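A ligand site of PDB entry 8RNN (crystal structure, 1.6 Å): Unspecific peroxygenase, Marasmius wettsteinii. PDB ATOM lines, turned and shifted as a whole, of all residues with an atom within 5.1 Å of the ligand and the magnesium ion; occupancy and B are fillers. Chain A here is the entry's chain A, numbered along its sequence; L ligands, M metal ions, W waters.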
ATOM      1  N   PRO A  20      31.188   1.699  17.329  1.00  0.00           N
ATOM      2  CA  PRO A  20      30.151   2.151  18.264  1.00  0.00           C
ATOM      3  C   PRO A  20      29.457   3.445  17.869  1.00  0.00           C
ATOM      4  O   PRO A  20      28.554   3.893  18.572  1.00  0.00           O
ATOM      5  CB  PRO A  20      30.998   2.317  19.538  1.00  0.00           C
ATOM      6  CG  PRO A  20      32.307   2.855  19.025  1.00  0.00           C
ATOM      7  CD  PRO A  20      32.542   2.099  17.741  1.00  0.00           C
ATOM      8  N   CYS A  21      29.869   4.015  16.719  1.00  0.00           N
ATOM      9  CA  CYS A  21      29.382   5.302  16.262  1.00  0.00           C
ATOM     10  C   CYS A  21      28.380   5.103  15.128  1.00  0.00           C
ATOM     11  O   CYS A  21      28.780   4.703  14.052  1.00  0.00           O
ATOM     12  CB  CYS A  21      30.519   6.174  15.774  1.00  0.00           C
ATOM     13  SG  CYS A  21      29.901   7.747  15.121  1.00  0.00           S
ATOM     14  N   PRO A  22      27.083   5.413  15.327  1.00  0.00           N
ATOM     15  CA  PRO A  22      26.102   5.328  14.239  1.00  0.00           C
ATOM     16  C   PRO A  22      26.390   6.316  13.117  1.00  0.00           C
ATOM     17  O   PRO A  22      26.026   6.077  11.954  1.00  0.00           O
ATOM     18  CB  PRO A  22      24.759   5.633  14.932  1.00  0.00           C
ATOM     19  CG  PRO A  22      25.161   6.495  16.109  1.00  0.00           C
ATOM     20  CD  PRO A  22      26.467   5.873  16.582  1.00  0.00           C
ATOM     21  N   GLY A  23      27.033   7.449  13.429  1.00  0.00           N
ATOM     22  CA  GLY A  23      27.336   8.441  12.397  1.00  0.00           C
ATOM     23  C   GLY A  23      28.295   7.876  11.367  1.00  0.00           C
ATOM     24  O   GLY A  23      28.024   7.923  10.149  1.00  0.00           O
ATOM     25  N   LEU A  24      29.424   7.328  11.798  1.00  0.00           N
ATOM     26  CA  LEU A  24      30.417   6.776  10.893  1.00  0.00           C
ATOM     27  C   LEU A  24      29.916   5.467  10.284  1.00  0.00           C
ATOM     28  O   LEU A  24      30.166   5.184   9.109  1.00  0.00           O
ATOM     29  CB  LEU A  24      31.725   6.582  11.655  1.00  0.00           C
ATOM     30  CG  LEU A  24      32.386   7.857  12.167  1.00  0.00           C
ATOM     31  CD1 LEU A  24      33.720   7.520  12.802  1.00  0.00           C
ATOM     32  CD2 LEU A  24      32.579   8.906  11.058  1.00  0.00           C
ATOM     33  N   ILE A  45      37.240  10.888   6.669  1.00  0.00           N
ATOM     34  CA  ILE A  45      36.127  11.180   7.557  1.00  0.00           C
ATOM     35  C   ILE A  45      35.584  12.601   7.300  1.00  0.00           C
ATOM     36  O   ILE A  45      34.392  12.825   7.247  1.00  0.00           O
ATOM     37  CB  ILE A  45      36.547  10.982   9.027  1.00  0.00           C
ATOM     38  CG1 ILE A  45      36.796   9.503   9.327  1.00  0.00           C
ATOM     39  CG2 ILE A  45      35.523  11.583   9.973  1.00  0.00           C
ATOM     40  CD1 ILE A  45      37.484   9.240  10.646  1.00  0.00           C
ATOM     41  N   TYR A  53      26.364  14.617   5.509  1.00  0.00           N
ATOM     42  CA  TYR A  53      25.621  15.233   6.590  1.00  0.00           C
ATOM     43  C   TYR A  53      25.766  16.761   6.653  1.00  0.00           C
ATOM     44  O   TYR A  53      25.042  17.406   7.421  1.00  0.00           O
ATOM     45  CB  TYR A  53      26.129  14.710   7.939  1.00  0.00           C
ATOM     46  CG  TYR A  53      26.050  13.228   8.208  1.00  0.00           C
ATOM     47  CD1 TYR A  53      24.940  12.471   7.852  1.00  0.00           C
ATOM     48  CD2 TYR A  53      27.057  12.578   8.909  1.00  0.00           C
ATOM     49  CE1 TYR A  53      24.853  11.126   8.160  1.00  0.00           C
ATOM     50  CE2 TYR A  53      26.984  11.227   9.225  1.00  0.00           C
ATOM     51  CZ  TYR A  53      25.873  10.499   8.853  1.00  0.00           C
ATOM     52  OH  TYR A  53      25.792   9.164   9.148  1.00  0.00           O
ATOM     53  N   VAL A  55      28.374  18.122   7.882  1.00  0.00           N
ATOM     54  CA  VAL A  55      29.159  18.378   9.082  1.00  0.00           C
ATOM     55  C   VAL A  55      30.532  18.869   8.645  1.00  0.00           C
ATOM     56  O   VAL A  55      31.156  18.289   7.765  1.00  0.00           O
ATOM     57  CB  VAL A  55      29.227  17.144  10.001  1.00  0.00           C
ATOM     58  CG1 VAL A  55      30.175  17.396  11.172  1.00  0.00           C
ATOM     59  CG2 VAL A  55      27.866  16.748  10.512  1.00  0.00           C
ATOM     60  N   ILE A  59      34.840  20.091  13.690  1.00  0.00           N
ATOM     61  CA  ILE A  59      34.554  19.033  14.657  1.00  0.00           C
ATOM     62  C   ILE A  59      35.150  17.705  14.182  1.00  0.00           C
ATOM     63  O   ILE A  59      35.600  16.899  15.010  1.00  0.00           O
ATOM     64  CB  ILE A  59      33.053  18.922  14.973  1.00  0.00           C
ATOM     65  CG1 ILE A  59      32.801  17.899  16.082  1.00  0.00           C
ATOM     66  CG2 ILE A  59      32.268  18.597  13.723  1.00  0.00           C
ATOM     67  CD1 ILE A  59      31.422  17.944  16.674  1.00  0.00           C
ATOM     68  N   LEU A  60      35.163  17.439  12.865  1.00  0.00           N
ATOM     69  CA  LEU A  60      35.608  16.143  12.370  1.00  0.00           C
ATOM     70  C   LEU A  60      37.128  15.975  12.456  1.00  0.00           C
ATOM     71  O   LEU A  60      37.605  14.866  12.683  1.00  0.00           O
ATOM     72  CB  LEU A  60      35.083  15.916  10.952  1.00  0.00           C
ATOM     73  CG  LEU A  60      33.564  15.843  10.837  1.00  0.00           C
ATOM     74  CD1 LEU A  60      33.137  15.669   9.395  1.00  0.00           C
ATOM     75  CD2 LEU A  60      32.981  14.716  11.681  1.00  0.00           C
ATOM     76  N   ALA A  63      37.663  15.447  16.512  1.00  0.00           N
ATOM     77  CA  ALA A  63      37.264  14.119  16.927  1.00  0.00           C
ATOM     78  C   ALA A  63      38.047  13.034  16.182  1.00  0.00           C
ATOM     79  O   ALA A  63      38.428  12.004  16.755  1.00  0.00           O
ATOM     80  CB  ALA A  63      35.783  13.940  16.717  1.00  0.00           C
ATOM     81  N   GLY A  64      38.272  13.250  14.892  1.00  0.00           N
ATOM     82  CA  GLY A  64      38.951  12.284  14.058  1.00  0.00           C
ATOM     83  C   GLY A  64      40.352  11.948  14.560  1.00  0.00           C
ATOM     84  O   GLY A  64      40.752  10.787  14.596  1.00  0.00           O
ATOM     85  N   GLY A  67      40.190   9.871  17.524  1.00  0.00           N
ATOM     86  CA  GLY A  67      39.842   8.520  17.114  1.00  0.00           C
ATOM     87  C   GLY A  67      41.021   7.741  16.527  1.00  0.00           C
ATOM     88  O   GLY A  67      41.121   6.531  16.701  1.00  0.00           O
ATOM     89  N   LEU A  82      37.368   2.018  17.152  1.00  0.00           N
ATOM     90  CA  LEU A  82      36.828   3.099  17.961  1.00  0.00           C
ATOM     91  C   LEU A  82      36.112   2.600  19.218  1.00  0.00           C
ATOM     92  O   LEU A  82      35.734   3.413  20.056  1.00  0.00           O
ATOM     93  CB  LEU A  82      35.862   3.926  17.092  1.00  0.00           C
ATOM     94  CG  LEU A  82      36.504   4.709  15.939  1.00  0.00           C
ATOM     95  CD1 LEU A  82      35.431   5.309  15.044  1.00  0.00           C
ATOM     96  CD2 LEU A  82      37.411   5.810  16.473  1.00  0.00           C
ATOM     97  N   ILE A  88      37.497   7.629  23.170  1.00  0.00           N
ATOM     98  CA  ILE A  88      36.212   8.294  23.018  1.00  0.00           C
ATOM     99  C   ILE A  88      35.114   7.439  23.650  1.00  0.00           C
ATOM    100  O   ILE A  88      34.249   7.958  24.351  1.00  0.00           O
ATOM    101  CB  ILE A  88      35.914   8.605  21.539  1.00  0.00           C
ATOM    102  CG1 ILE A  88      36.955   9.557  20.966  1.00  0.00           C
ATOM    103  CG2 ILE A  88      34.500   9.153  21.368  1.00  0.00           C
ATOM    104  CD1 ILE A  88      36.910   9.678  19.447  1.00  0.00           C
ATOM    105  N   GLU A  89      35.136   6.125  23.370  1.00  0.00           N
ATOM    106  CA  GLU A  89      34.070   5.248  23.842  1.00  0.00           C
ATOM    107  C   GLU A  89      33.942   5.355  25.374  1.00  0.00           C
ATOM    108  O   GLU A  89      34.942   5.390  26.088  1.00  0.00           O
ATOM    109  CB  GLU A  89      34.302   3.809  23.385  1.00  0.00           C
ATOM    110  CG  GLU A  89      33.068   2.937  23.541  1.00  0.00           C
ATOM    111  CD  GLU A  89      32.784   2.483  24.963  1.00  0.00           C
ATOM    112  OE1 GLU A  89      33.760   2.127  25.671  1.00  0.00           O
ATOM    113  OE2 GLU A  89      31.604   2.460  25.350  1.00  0.00           O
ATOM    114  N   HIS A  90      32.691   5.457  25.829  1.00  0.00           N
ATOM    115  CA  HIS A  90      32.360   5.766  27.218  1.00  0.00           C
ATOM    116  C   HIS A  90      31.133   4.983  27.682  1.00  0.00           C
ATOM    117  O   HIS A  90      30.319   4.478  26.890  1.00  0.00           O
ATOM    118  CB  HIS A  90      32.071   7.277  27.352  1.00  0.00           C
ATOM    119  CG  HIS A  90      31.029   7.742  26.390  1.00  0.00           C
ATOM    120  ND1 HIS A  90      29.688   7.465  26.549  1.00  0.00           N
ATOM    121  CD2 HIS A  90      31.136   8.431  25.232  1.00  0.00           C
ATOM    122  CE1 HIS A  90      29.013   7.951  25.511  1.00  0.00           C
ATOM    123  NE2 HIS A  90      29.873   8.539  24.704  1.00  0.00           N
ATOM    124  N   ASP A  91      30.954   4.939  29.002  1.00  0.00           N
ATOM    125  CA  ASP A  91      29.760   4.399  29.613  1.00  0.00           C
ATOM    126  C   ASP A  91      28.560   5.317  29.393  1.00  0.00           C
ATOM    127  O   ASP A  91      28.720   6.470  28.976  1.00  0.00           O
ATOM    128  CB  ASP A  91      30.024   4.217  31.108  1.00  0.00           C
ATOM    129  CG  ASP A  91      31.140   3.245  31.400  1.00  0.00           C
ATOM    130  OD1 ASP A  91      31.363   2.343  30.586  1.00  0.00           O
ATOM    131  OD2 ASP A  91      31.781   3.397  32.467  1.00  0.00           O
ATOM    132  N   SER A  93      26.183   5.131  27.170  1.00  0.00           N
ATOM    133  CA  SER A  93      25.846   5.338  25.772  1.00  0.00           C
ATOM    134  C   SER A  93      24.332   5.270  25.602  1.00  0.00           C
ATOM    135  O   SER A  93      23.625   4.726  26.456  1.00  0.00           O
ATOM    136  CB  SER A  93      26.531   4.327  24.892  1.00  0.00           C
ATOM    137  OG  SER A  93      27.937   4.521  24.857  1.00  0.00           O
ATOM    138  N   LEU A  94      23.835   5.789  24.471  1.00  0.00           N
ATOM    139  CA  LEU A  94      22.408   5.838  24.142  1.00  0.00           C
ATOM    140  C   LEU A  94      21.891   4.503  23.605  1.00  0.00           C
ATOM    141  O   LEU A  94      20.679   4.266  23.651  1.00  0.00           O
ATOM    142  CB  LEU A  94      22.175   6.922  23.093  1.00  0.00           C
ATOM    143  CG  LEU A  94      22.568   8.344  23.490  1.00  0.00           C
ATOM    144  CD1 LEU A  94      22.671   9.253  22.261  1.00  0.00           C
ATOM    145  CD2 LEU A  94      21.605   8.896  24.502  1.00  0.00           C
ATOM    146  N   SER A  95      22.766   3.699  23.016  1.00  0.00           N
ATOM    147  CA  SER A  95      22.329   2.534  22.259  1.00  0.00           C
ATOM    148  C   SER A  95      23.280   1.337  22.404  1.00  0.00           C
ATOM    149  O   SER A  95      23.064   0.324  21.752  1.00  0.00           O
ATOM    150  CB  SER A  95      22.139   2.905  20.795  1.00  0.00           C
ATOM    151  OG  SER A  95      23.373   3.136  20.126  1.00  0.00           O
ATOM    152  N   ARG A  96      24.322   1.480  23.235  1.00  0.00           N
ATOM    153  CA  ARG A  96      25.290   0.427  23.506  1.00  0.00           C
ATOM    154  C   ARG A  96      25.336   0.179  25.006  1.00  0.00           C
ATOM    155  O   ARG A  96      24.980   1.054  25.785  1.00  0.00           O
ATOM    156  CB  ARG A  96      26.696   0.795  23.020  1.00  0.00           C
ATOM    157  CG  ARG A  96      27.041   0.453  21.581  1.00  0.00           C
ATOM    158  CD  ARG A  96      26.162   1.084  20.536  1.00  0.00           C
ATOM    159  NE  ARG A  96      26.686   0.840  19.201  1.00  0.00           N
ATOM    160  CZ  ARG A  96      26.063   1.152  18.067  1.00  0.00           C
ATOM    161  NH1 ARG A  96      24.923   1.811  18.078  1.00  0.00           N
ATOM    162  NH2 ARG A  96      26.616   0.792  16.924  1.00  0.00           N
ATOM    163  N   GLU A  97      25.848  -0.993  25.414  1.00  0.00           N
ATOM    164  CA  GLU A  97      26.039  -1.309  26.816  1.00  0.00           C
ATOM    165  C   GLU A  97      27.409  -0.816  27.280  1.00  0.00           C
ATOM    166  O   GLU A  97      28.307  -0.603  26.469  1.00  0.00           O
ATOM    167  CB  GLU A  97      25.927  -2.817  27.024  1.00  0.00           C
ATOM    168  CG  GLU A  97      24.572  -3.381  26.631  1.00  0.00           C
ATOM    169  CD  GLU A  97      24.435  -4.887  26.647  1.00  0.00           C
ATOM    170  OE1 GLU A  97      25.447  -5.601  26.447  1.00  0.00           O
ATOM    171  OE2 GLU A  97      23.294  -5.350  26.915  1.00  0.00           O
ATOM    172  N   ASN A 104      29.981  -3.081  24.244  1.00  0.00           N
ATOM    173  CA  ASN A 104      30.108  -1.648  24.066  1.00  0.00           C
ATOM    174  C   ASN A 104      30.201  -1.270  22.591  1.00  0.00           C
ATOM    175  O   ASN A 104      30.491  -0.110  22.297  1.00  0.00           O
ATOM    176  CB  ASN A 104      31.324  -1.087  24.819  1.00  0.00           C
ATOM    177  CG  ASN A 104      32.650  -1.383  24.149  1.00  0.00           C
ATOM    178  OD1 ASN A 104      32.756  -2.301  23.357  1.00  0.00           O
ATOM    179  ND2 ASN A 104      33.676  -0.602  24.450  1.00  0.00           N
ATOM    180  N   GLU A 161      27.293  13.982  21.268  1.00  0.00           N
ATOM    181  CA  GLU A 161      26.676  12.907  20.509  1.00  0.00           C
ATOM    182  C   GLU A 161      25.163  13.134  20.380  1.00  0.00           C
ATOM    183  O   GLU A 161      24.586  12.895  19.323  1.00  0.00           O
ATOM    184  CB  GLU A 161      27.087  11.570  21.141  1.00  0.00           C
ATOM    185  CG  GLU A 161      28.544  11.272  20.878  1.00  0.00           C
ATOM    186  CD  GLU A 161      29.268  10.296  21.794  1.00  0.00           C
ATOM    187  OE1 GLU A 161      28.658   9.841  22.754  1.00  0.00           O
ATOM    188  OE2 GLU A 161      30.465  10.022  21.499  1.00  0.00           O
ATOM    189  N   PHE A 164      24.622  15.733  17.876  1.00  0.00           N
ATOM    190  CA  PHE A 164      24.776  15.177  16.535  1.00  0.00           C
ATOM    191  C   PHE A 164      23.463  14.541  16.051  1.00  0.00           C
ATOM    192  O   PHE A 164      23.050  14.823  14.921  1.00  0.00           O
ATOM    193  CB  PHE A 164      25.922  14.159  16.461  1.00  0.00           C
ATOM    194  CG  PHE A 164      27.257  14.701  16.004  1.00  0.00           C
ATOM    195  CD1 PHE A 164      27.319  15.633  14.981  1.00  0.00           C
ATOM    196  CD2 PHE A 164      28.440  14.117  16.449  1.00  0.00           C
ATOM    197  CE1 PHE A 164      28.541  16.082  14.506  1.00  0.00           C
ATOM    198  CE2 PHE A 164      29.666  14.563  15.953  1.00  0.00           C
ATOM    199  CZ  PHE A 164      29.712  15.539  14.978  1.00  0.00           C
ATOM    200  N   TYR A 165      22.807  13.681  16.845  1.00  0.00           N
ATOM    201  CA  TYR A 165      21.598  13.056  16.322  1.00  0.00           C
ATOM    202  C   TYR A 165      20.510  14.095  16.104  1.00  0.00           C
ATOM    203  O   TYR A 165      19.759  13.989  15.130  1.00  0.00           O
ATOM    204  CB  TYR A 165      21.163  11.816  17.118  1.00  0.00           C
ATOM    205  CG  TYR A 165      20.415  12.009  18.414  1.00  0.00           C
ATOM    206  CD1 TYR A 165      19.107  12.464  18.464  1.00  0.00           C
ATOM    207  CD2 TYR A 165      21.006  11.635  19.610  1.00  0.00           C
ATOM    208  CE1 TYR A 165      18.415  12.597  19.652  1.00  0.00           C
ATOM    209  CE2 TYR A 165      20.331  11.763  20.816  1.00  0.00           C
ATOM    210  CZ  TYR A 165      19.032  12.238  20.839  1.00  0.00           C
ATOM    211  OH  TYR A 165      18.379  12.380  22.025  1.00  0.00           O
ATOM    212  N   VAL A 168      22.028  16.280  12.652  1.00  0.00           N
ATOM    213  CA  VAL A 168      22.284  15.633  11.375  1.00  0.00           C
ATOM    214  C   VAL A 168      21.008  14.989  10.830  1.00  0.00           C
ATOM    215  O   VAL A 168      20.823  14.933   9.609  1.00  0.00           O
ATOM    216  CB  VAL A 168      23.443  14.621  11.495  1.00  0.00           C
ATOM    217  CG1 VAL A 168      23.578  13.762  10.266  1.00  0.00           C
ATOM    218  CG2 VAL A 168      24.759  15.311  11.812  1.00  0.00           C
ATOM    219  N   PHE A 187      18.232   5.905  11.885  1.00  0.00           N
ATOM    220  CA  PHE A 187      19.655   6.184  12.008  1.00  0.00           C
ATOM    221  C   PHE A 187      20.323   5.212  12.990  1.00  0.00           C
ATOM    222  O   PHE A 187      21.336   4.589  12.679  1.00  0.00           O
ATOM    223  CB  PHE A 187      19.800   7.650  12.428  1.00  0.00           C
ATOM    224  CG  PHE A 187      21.204   8.136  12.675  1.00  0.00           C
ATOM    225  CD1 PHE A 187      22.120   8.225  11.652  1.00  0.00           C
ATOM    226  CD2 PHE A 187      21.588   8.517  13.944  1.00  0.00           C
ATOM    227  CE1 PHE A 187      23.403   8.699  11.880  1.00  0.00           C
ATOM    228  CE2 PHE A 187      22.874   8.982  14.173  1.00  0.00           C
ATOM    229  CZ  PHE A 187      23.781   9.057  13.144  1.00  0.00           C
ATOM    230  N   PHE A 188      19.758   5.077  14.195  1.00  0.00           N
ATOM    231  CA  PHE A 188      20.303   4.205  15.231  1.00  0.00           C
ATOM    232  C   PHE A 188      20.053   2.724  14.914  1.00  0.00           C
ATOM    233  O   PHE A 188      20.958   1.910  14.969  1.00  0.00           O
ATOM    234  CB  PHE A 188      19.722   4.563  16.601  1.00  0.00           C
ATOM    235  CG  PHE A 188      20.397   5.693  17.346  1.00  0.00           C
ATOM    236  CD1 PHE A 188      21.517   5.454  18.122  1.00  0.00           C
ATOM    237  CD2 PHE A 188      19.911   6.993  17.264  1.00  0.00           C
ATOM    238  CE1 PHE A 188      22.124   6.499  18.826  1.00  0.00           C
ATOM    239  CE2 PHE A 188      20.520   8.029  17.969  1.00  0.00           C
ATOM    240  CZ  PHE A 188      21.633   7.766  18.741  1.00  0.00           C
HETATM  241  C1  LIG L   1      29.180   7.732  19.339  1.00  0.00           C
HETATM  242  C2  LIG L   1      33.465   8.422  17.290  1.00  0.00           C
HETATM  243  C3  LIG L   1      31.467  11.387  14.042  1.00  0.00           C
HETATM  244  C4  LIG L   1      27.152  10.518  15.963  1.00  0.00           C
HETATM  245  C5  LIG L   1      30.499   7.623  19.035  1.00  0.00           C
HETATM  246  C6  LIG L   1      31.430   6.795  19.714  1.00  0.00           C
HETATM  247  C7  LIG L   1      32.648   6.971  19.133  1.00  0.00           C
HETATM  248  C8  LIG L   1      32.463   7.920  18.075  1.00  0.00           C
HETATM  249  C9  LIG L   1      33.928   6.277  19.501  1.00  0.00           C
HETATM  250  C10 LIG L   1      31.084   5.868  20.861  1.00  0.00           C
HETATM  251  C11 LIG L   1      30.846   6.686  22.145  1.00  0.00           C
HETATM  252  C12 LIG L   1      29.973   5.911  23.062  1.00  0.00           C
HETATM  253  O1  LIG L   1      28.741   5.947  22.917  1.00  0.00           O
HETATM  254  O2  LIG L   1      30.498   5.194  23.960  1.00  0.00           O
HETATM  255  C13 LIG L   1      33.304   9.361  16.270  1.00  0.00           C
HETATM  256  C14 LIG L   1      34.401   9.870  15.523  1.00  0.00           C
HETATM  257  C15 LIG L   1      33.830  10.684  14.577  1.00  0.00           C
HETATM  258  C16 LIG L   1      32.387  10.681  14.807  1.00  0.00           C
HETATM  259  C17 LIG L   1      35.858   9.556  15.651  1.00  0.00           C
HETATM  260  C18 LIG L   1      34.615  11.532  13.669  1.00  0.00           C
HETATM  261  C19 LIG L   1      34.284  12.781  13.609  1.00  0.00           C
HETATM  262  C20 LIG L   1      30.111  11.346  14.215  1.00  0.00           C
HETATM  263  C21 LIG L   1      29.154  11.953  13.394  1.00  0.00           C
HETATM  264  C22 LIG L   1      27.931  11.740  13.931  1.00  0.00           C
HETATM  265  C23 LIG L   1      28.112  10.940  15.120  1.00  0.00           C
HETATM  266  C24 LIG L   1      29.432  12.746  12.132  1.00  0.00           C
HETATM  267  C25 LIG L   1      26.693  12.180  13.263  1.00  0.00           C
HETATM  268  C26 LIG L   1      25.672  11.400  13.307  1.00  0.00           C
HETATM  269  C27 LIG L   1      27.379   9.712  17.089  1.00  0.00           C
HETATM  270  C28 LIG L   1      26.285   9.362  18.037  1.00  0.00           C
HETATM  271  C29 LIG L   1      26.867   8.569  18.966  1.00  0.00           C
HETATM  272  C30 LIG L   1      28.284   8.497  18.589  1.00  0.00           C
HETATM  273  C31 LIG L   1      24.816   9.763  17.970  1.00  0.00           C
HETATM  274  C32 LIG L   1      26.251   7.950  20.219  1.00  0.00           C
HETATM  275  C33 LIG L   1      25.976   6.460  20.140  1.00  0.00           C
HETATM  276  C34 LIG L   1      25.440   5.974  21.475  1.00  0.00           C
HETATM  277  O3  LIG L   1      24.893   4.859  21.544  1.00  0.00           O
HETATM  278  O4  LIG L   1      25.514   6.715  22.495  1.00  0.00           O
HETATM  279  N1  LIG L   1      31.171   8.327  18.035  1.00  0.00           N
HETATM  280  N2  LIG L   1      32.145   9.860  15.845  1.00  0.00           N
HETATM  281  N3  LIG L   1      29.462  10.741  15.222  1.00  0.00           N
HETATM  282  N4  LIG L   1      28.566   9.202  17.457  1.00  0.00           N
HETATM  283 FE1  LIG L   1      30.270   9.427  16.608  1.00  0.00          FE
HETATM  284 MG    MG M   1      29.833   3.488  25.078  1.00  0.00          MG
HETATM  285  O   HOH W   1      26.332   8.891  23.882  1.00  0.00           O
HETATM  286  O   HOH W   2      29.587   2.448  23.213  1.00  0.00           O
HETATM  287  O   HOH W   3      28.794   2.069  26.258  1.00  0.00           O
HETATM  288  O   HOH W   4      28.107   3.627  21.320  1.00  0.00           O
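N of His 90 sits close to O2 of the ligand. An oxygen (O1) of the ligand sits close to a ring nitrogen (NE2) of His 90 (3.3 Å). FE1 of the ligand is bound by SG of Cys 21. An oxygen (O3) of the ligand lies within hydrogen-bond range of the backbone NH of Ser 95 (2.8 Å). An oxygen (O3) of the ligand lies within hydrogen-bond range of the side-chain hydroxyl of Ser 95, 2.7 Å away. N of Leu 94 lies within hydrogen-bond range of O4 of the ligand.
CG of Pro 20 touches C10 of the ligand, 3.7 Å away. CD of Pro 22 touches C29 of the ligand, at 3.6 Å. CA of Gly 23 touches C26 of the ligand, at 3.5 Å. CD1 of Leu 24 touches C15 of the ligand, at 3.6 Å. Ile 45 touches the ligand (CG2 to C18, 3.8 Å). CD2 of Leu 60 touches C19 of the ligand, at 3.0 Å. Ala 63 touches the ligand. Leu 82 touches the ligand. Ile 88 touches the ligand (CG2 to C9, 3.5 Å). N of Arg 96 touches O3 of the ligand, at 3.8 Å. OE2 of Glu 161 touches C1 of the ligand (3.4 Å). Phe 164 touches the ligand (CD2 to C23, 3.5 Å). CG2 of Val 168 touches C25 of the ligand, at 3.96 Å. Phe 187 touches the ligand (CZ to C26, 3.0 Å). CZ of Phe 188 touches C31 of the ligand, at 3.8 Å. Of the 30 residues printed, 21 come within 4 Å of the ligand. The nearest printed residue that does not touch the ligand is Tyr 53 (4.01 Å).
Of the 30 residues printed, 3 come within 4 Å of the magnesium ion. The nearest printed residue that does not touch the magnesium ion is Asp 91 (4.3 Å).
The magnesium ion is bound by the side-chain carboxylate (OE2) of Glu 89 (2.1 Å), water W3 (2.1 Å), the backbone carbonyl oxygen (O) of His 90 (2.1 Å), an oxygen (O2) of the ligand (2.1 Å), water W2 (2.1 Å) and the side-chain hydroxyl (OG) of Ser 93 (2.2 Å). The magnesium ion has six donor atoms within binding distance.
Water W1 bridges an oxygen (O4) of the ligand (2.7 Å) and the side-chain carboxylate (OE1) of Glu 161 (2.8 Å). Water W4 lies within hydrogen-bond range of O of Pro 20 and O1 of the ligand.
The side-chain carboxylate (OE1) of Glu 89 lies within hydrogen-bond range of the side-chain amide nitrogen (ND2) of Asn 104 (3.0 Å). A ring nitrogen (NE2) of His 90 lies within hydrogen-bond range of the side-chain carboxylate (OE1) of Glu 161 (2.6 Å). The side-chain sulfur (SG) of Cys 21 lies close to the backbone NH (N) of Gly 23. N of Leu 24 lies close to SG of Cys 21, 3.4 Å away. OG of Ser 95 sits at hydrogen-bond distance from NH1 of Arg 96, 2.9 Å away. O of Gly 23 lies within hydrogen-bond range of OH of Tyr 53, at 2.7 Å.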
